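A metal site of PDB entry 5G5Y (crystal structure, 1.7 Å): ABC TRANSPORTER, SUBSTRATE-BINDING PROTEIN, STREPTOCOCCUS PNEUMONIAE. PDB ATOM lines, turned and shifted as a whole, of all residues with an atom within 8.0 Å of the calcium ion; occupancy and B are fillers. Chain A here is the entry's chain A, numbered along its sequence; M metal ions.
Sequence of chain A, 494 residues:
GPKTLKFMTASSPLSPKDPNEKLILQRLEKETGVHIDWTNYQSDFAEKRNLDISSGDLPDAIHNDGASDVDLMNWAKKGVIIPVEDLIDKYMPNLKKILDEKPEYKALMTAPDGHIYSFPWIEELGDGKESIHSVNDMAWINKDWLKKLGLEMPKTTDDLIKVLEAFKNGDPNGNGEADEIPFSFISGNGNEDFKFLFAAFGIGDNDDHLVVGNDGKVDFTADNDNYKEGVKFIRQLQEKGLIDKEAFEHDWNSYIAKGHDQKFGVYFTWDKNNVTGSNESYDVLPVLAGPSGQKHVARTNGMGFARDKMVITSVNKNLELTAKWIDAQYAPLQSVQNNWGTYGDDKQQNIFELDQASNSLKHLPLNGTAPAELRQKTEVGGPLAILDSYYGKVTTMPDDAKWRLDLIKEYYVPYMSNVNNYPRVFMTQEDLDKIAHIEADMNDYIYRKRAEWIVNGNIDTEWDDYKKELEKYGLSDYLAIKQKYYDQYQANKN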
ATOM      1  N   TRP A 145      -1.650 -22.816  21.241  1.00  0.00           N
ATOM      2  CA  TRP A 145      -1.667 -21.790  22.325  1.00  0.00           C
ATOM      3  C   TRP A 145      -2.723 -20.699  22.107  1.00  0.00           C
ATOM      4  O   TRP A 145      -3.424 -20.309  23.048  1.00  0.00           O
ATOM      5  CB  TRP A 145      -0.290 -21.161  22.511  1.00  0.00           C
ATOM      6  CG  TRP A 145       0.759 -22.104  22.956  1.00  0.00           C
ATOM      7  CD1 TRP A 145       0.657 -23.453  23.156  1.00  0.00           C
ATOM      8  CD2 TRP A 145       2.115 -21.766  23.253  1.00  0.00           C
ATOM      9  NE1 TRP A 145       1.843 -23.969  23.556  1.00  0.00           N
ATOM     10  CE2 TRP A 145       2.761 -22.958  23.627  1.00  0.00           C
ATOM     11  CE3 TRP A 145       2.826 -20.575  23.244  1.00  0.00           C
ATOM     12  CZ2 TRP A 145       4.089 -22.990  23.975  1.00  0.00           C
ATOM     13  CZ3 TRP A 145       4.163 -20.620  23.576  1.00  0.00           C
ATOM     14  CH2 TRP A 145       4.773 -21.797  23.942  1.00  0.00           C
ATOM     15  N   PHE A 167       0.975 -15.545  25.985  1.00  0.00           N
ATOM     16  CA  PHE A 167       1.835 -16.727  25.951  1.00  0.00           C
ATOM     17  C   PHE A 167       2.802 -16.762  27.143  1.00  0.00           C
ATOM     18  O   PHE A 167       3.081 -17.830  27.691  1.00  0.00           O
ATOM     19  CB  PHE A 167       2.719 -16.774  24.682  1.00  0.00           C
ATOM     20  CG  PHE A 167       1.981 -17.001  23.388  1.00  0.00           C
ATOM     21  CD1 PHE A 167       0.636 -17.420  23.327  1.00  0.00           C
ATOM     22  CD2 PHE A 167       2.685 -16.877  22.192  1.00  0.00           C
ATOM     23  CE1 PHE A 167       0.018 -17.633  22.108  1.00  0.00           C
ATOM     24  CE2 PHE A 167       2.067 -17.115  20.975  1.00  0.00           C
ATOM     25  CZ  PHE A 167       0.743 -17.504  20.922  1.00  0.00           C
ATOM     26  N   LYS A 168       3.360 -15.618  27.508  1.00  0.00           N
ATOM     27  CA  LYS A 168       4.315 -15.565  28.618  1.00  0.00           C
ATOM     28  C   LYS A 168       3.647 -15.960  29.949  1.00  0.00           C
ATOM     29  O   LYS A 168       4.197 -16.764  30.680  1.00  0.00           O
ATOM     30  CB  LYS A 168       4.942 -14.171  28.747  1.00  0.00           C
ATOM     31  CG  LYS A 168       6.162 -14.070  29.668  1.00  0.00           C
ATOM     32  CD  LYS A 168       6.467 -12.604  29.966  1.00  0.00           C
ATOM     33  CE  LYS A 168       7.251 -12.394  31.226  1.00  0.00           C
ATOM     34  NZ  LYS A 168       8.614 -12.960  31.090  1.00  0.00           N
ATOM     35  N   ASN A 169       2.496 -15.356  30.229  1.00  0.00           N
ATOM     36  CA  ASN A 169       1.865 -15.410  31.559  1.00  0.00           C
ATOM     37  C   ASN A 169       0.703 -16.376  31.662  1.00  0.00           C
ATOM     38  O   ASN A 169       0.238 -16.650  32.763  1.00  0.00           O
ATOM     39  CB  ASN A 169       1.318 -14.021  31.922  1.00  0.00           C
ATOM     40  CG  ASN A 169       2.386 -12.933  31.864  1.00  0.00           C
ATOM     41  OD1 ASN A 169       3.518 -13.148  32.260  1.00  0.00           O
ATOM     42  ND2 ASN A 169       2.010 -11.754  31.356  1.00  0.00           N
ATOM     43  N   GLY A 170       0.173 -16.837  30.533  1.00  0.00           N
ATOM     44  CA  GLY A 170      -1.085 -17.594  30.510  1.00  0.00           C
ATOM     45  C   GLY A 170      -0.967 -19.095  30.594  1.00  0.00           C
ATOM     46  O   GLY A 170      -1.986 -19.783  30.562  1.00  0.00           O
ATOM     47  N   ASP A 171       0.246 -19.625  30.638  1.00  0.00           N
ATOM     48  CA  ASP A 171       0.483 -21.061  30.657  1.00  0.00           C
ATOM     49  C   ASP A 171      -0.391 -21.831  29.617  1.00  0.00           C
ATOM     50  O   ASP A 171      -1.160 -22.727  29.987  1.00  0.00           O
ATOM     51  CB  ASP A 171       0.316 -21.609  32.083  1.00  0.00           C
ATOM     52  CG  ASP A 171       0.665 -23.087  32.206  1.00  0.00           C
ATOM     53  OD1 ASP A 171       1.670 -23.526  31.572  1.00  0.00           O
ATOM     54  OD2 ASP A 171      -0.059 -23.815  32.942  1.00  0.00           O
ATOM     55  N   PRO A 172      -0.249 -21.488  28.322  1.00  0.00           N
ATOM     56  CA  PRO A 172      -1.086 -22.172  27.317  1.00  0.00           C
ATOM     57  C   PRO A 172      -0.831 -23.685  27.183  1.00  0.00           C
ATOM     58  O   PRO A 172      -1.756 -24.408  26.798  1.00  0.00           O
ATOM     59  CB  PRO A 172      -0.742 -21.446  26.004  1.00  0.00           C
ATOM     60  CG  PRO A 172       0.590 -20.814  26.244  1.00  0.00           C
ATOM     61  CD  PRO A 172       0.519 -20.385  27.704  1.00  0.00           C
ATOM     62  N   ASN A 173       0.356 -24.175  27.490  1.00  0.00           N
ATOM     63  CA  ASN A 173       0.554 -25.633  27.451  1.00  0.00           C
ATOM     64  C   ASN A 173       0.050 -26.367  28.730  1.00  0.00           C
ATOM     65  O   ASN A 173       0.224 -27.569  28.848  1.00  0.00           O
ATOM     66  CB  ASN A 173       2.002 -26.012  27.091  1.00  0.00           C
ATOM     67  CG  ASN A 173       2.987 -25.789  28.224  1.00  0.00           C
ATOM     68  OD1 ASN A 173       2.613 -25.440  29.344  1.00  0.00           O
ATOM     69  ND2 ASN A 173       4.263 -25.981  27.930  1.00  0.00           N
ATOM     70  N   GLY A 174      -0.521 -25.615  29.685  1.00  0.00           N
ATOM     71  CA  GLY A 174      -1.284 -26.195  30.783  1.00  0.00           C
ATOM     72  C   GLY A 174      -0.514 -26.971  31.835  1.00  0.00           C
ATOM     73  O   GLY A 174      -1.131 -27.704  32.622  1.00  0.00           O
ATOM     74  N   ASN A 175       0.813 -26.811  31.909  1.00  0.00           N
ATOM     75  CA  ASN A 175       1.627 -27.551  32.885  1.00  0.00           C
ATOM     76  C   ASN A 175       1.926 -26.765  34.185  1.00  0.00           C
ATOM     77  O   ASN A 175       2.831 -27.113  34.931  1.00  0.00           O
ATOM     78  CB  ASN A 175       2.908 -28.069  32.210  1.00  0.00           C
ATOM     79  CG  ASN A 175       3.871 -26.942  31.788  1.00  0.00           C
ATOM     80  OD1 ASN A 175       3.631 -25.770  32.071  1.00  0.00           O
ATOM     81  ND2 ASN A 175       4.954 -27.315  31.120  1.00  0.00           N
ATOM     82  N   GLY A 176       1.179 -25.685  34.448  1.00  0.00           N
ATOM     83  CA  GLY A 176       1.426 -24.809  35.607  1.00  0.00           C
ATOM     84  C   GLY A 176       2.813 -24.177  35.758  1.00  0.00           C
ATOM     85  O   GLY A 176       3.132 -23.669  36.834  1.00  0.00           O
ATOM     86  N   GLU A 177       3.632 -24.183  34.693  1.00  0.00           N
ATOM     87  CA  GLU A 177       4.980 -23.587  34.714  1.00  0.00           C
ATOM     88  C   GLU A 177       5.088 -22.437  33.712  1.00  0.00           C
ATOM     89  O   GLU A 177       4.362 -22.434  32.703  1.00  0.00           O
ATOM     90  CB  GLU A 177       6.048 -24.604  34.324  1.00  0.00           C
ATOM     91  CG  GLU A 177       6.123 -25.839  35.207  1.00  0.00           C
ATOM     92  CD  GLU A 177       7.290 -26.761  34.837  1.00  0.00           C
ATOM     93  OE1 GLU A 177       8.005 -26.486  33.845  1.00  0.00           O
ATOM     94  OE2 GLU A 177       7.498 -27.766  35.554  1.00  0.00           O
ATOM     95  N   ALA A 178       6.016 -21.511  33.965  1.00  0.00           N
ATOM     96  CA  ALA A 178       6.353 -20.429  33.039  1.00  0.00           C
ATOM     97  C   ALA A 178       7.500 -20.900  32.130  1.00  0.00           C
ATOM     98  O   ALA A 178       8.604 -20.346  32.134  1.00  0.00           O
ATOM     99  CB  ALA A 178       6.742 -19.164  33.800  1.00  0.00           C
ATOM    100  N   ASP A 179       7.215 -21.941  31.355  1.00  0.00           N
ATOM    101  CA  ASP A 179       8.179 -22.546  30.433  1.00  0.00           C
ATOM    102  C   ASP A 179       8.043 -22.027  28.981  1.00  0.00           C
ATOM    103  O   ASP A 179       8.941 -22.205  28.168  1.00  0.00           O
ATOM    104  CB  ASP A 179       8.065 -24.071  30.478  1.00  0.00           C
ATOM    105  CG  ASP A 179       6.709 -24.602  30.002  1.00  0.00           C
ATOM    106  OD1 ASP A 179       5.613 -24.029  30.277  1.00  0.00           O
ATOM    107  OD2 ASP A 179       6.720 -25.677  29.365  1.00  0.00           O
ATOM    108  N   GLU A 180       6.921 -21.361  28.695  1.00  0.00           N
ATOM    109  CA  GLU A 180       6.654 -20.826  27.354  1.00  0.00           C
ATOM    110  C   GLU A 180       7.712 -19.747  27.006  1.00  0.00           C
ATOM    111  O   GLU A 180       7.987 -18.842  27.821  1.00  0.00           O
ATOM    112  CB  GLU A 180       5.239 -20.245  27.276  1.00  0.00           C
ATOM    113  CG  GLU A 180       4.092 -21.258  27.234  1.00  0.00           C
ATOM    114  CD  GLU A 180       3.621 -21.799  28.604  1.00  0.00           C
ATOM    115  OE1 GLU A 180       4.172 -21.392  29.649  1.00  0.00           O
ATOM    116  OE2 GLU A 180       2.670 -22.640  28.634  1.00  0.00           O
ATOM    117  N   ILE A 181       8.326 -19.887  25.836  1.00  0.00           N
ATOM    118  CA  ILE A 181       9.267 -18.908  25.300  1.00  0.00           C
ATOM    119  C   ILE A 181       8.454 -18.161  24.241  1.00  0.00           C
ATOM    120  O   ILE A 181       8.200 -18.719  23.183  1.00  0.00           O
ATOM    121  CB  ILE A 181      10.499 -19.571  24.679  1.00  0.00           C
ATOM    122  CG1 ILE A 181      11.215 -20.466  25.714  1.00  0.00           C
ATOM    123  CG2 ILE A 181      11.473 -18.504  24.153  1.00  0.00           C
ATOM    124  CD1 ILE A 181      12.353 -21.287  25.175  1.00  0.00           C
ATOM    125  N   LYS A 263       8.309 -25.305  22.641  1.00  0.00           N
ATOM    126  CA  LYS A 263       8.444 -24.262  23.673  1.00  0.00           C
ATOM    127  C   LYS A 263       8.230 -22.839  23.129  1.00  0.00           C
ATOM    128  O   LYS A 263       8.083 -21.876  23.913  1.00  0.00           O
ATOM    129  CB  LYS A 263       9.803 -24.375  24.349  1.00  0.00           C
ATOM    130  CG  LYS A 263       9.983 -25.655  25.180  1.00  0.00           C
ATOM    131  CD  LYS A 263       9.187 -25.585  26.484  1.00  0.00           C
ATOM    132  CE  LYS A 263       9.168 -26.901  27.260  1.00  0.00           C
ATOM    133  NZ  LYS A 263      10.534 -27.488  27.396  1.00  0.00           N
HETATM  134 CA    CA M   1       3.588 -23.684  30.776  1.00  0.00          CA
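The backbone NH (N) of Gly 176 lies within hydrogen-bond range of the side-chain carboxylate (OD2) of Asp 171 (2.7 Å).
Within 4 Å of the calcium ion: Asp 171, Asn 173, Asn 175, Glu 177, Asp 179 and Glu 180. Along chain A the residues within 4 Å of the calcium ion span positions 171 to 180. The nearest printed residue that does not touch the calcium ion is Ala 178 (4.6 Å).
The calcium ion is bound by OD1 of Asp 171, OD1 of Asp 179, O of Glu 177, OD1 of Asn 175, OD1 of Asn 173, OE2 of Glu 180 and OE1 of Glu 180.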
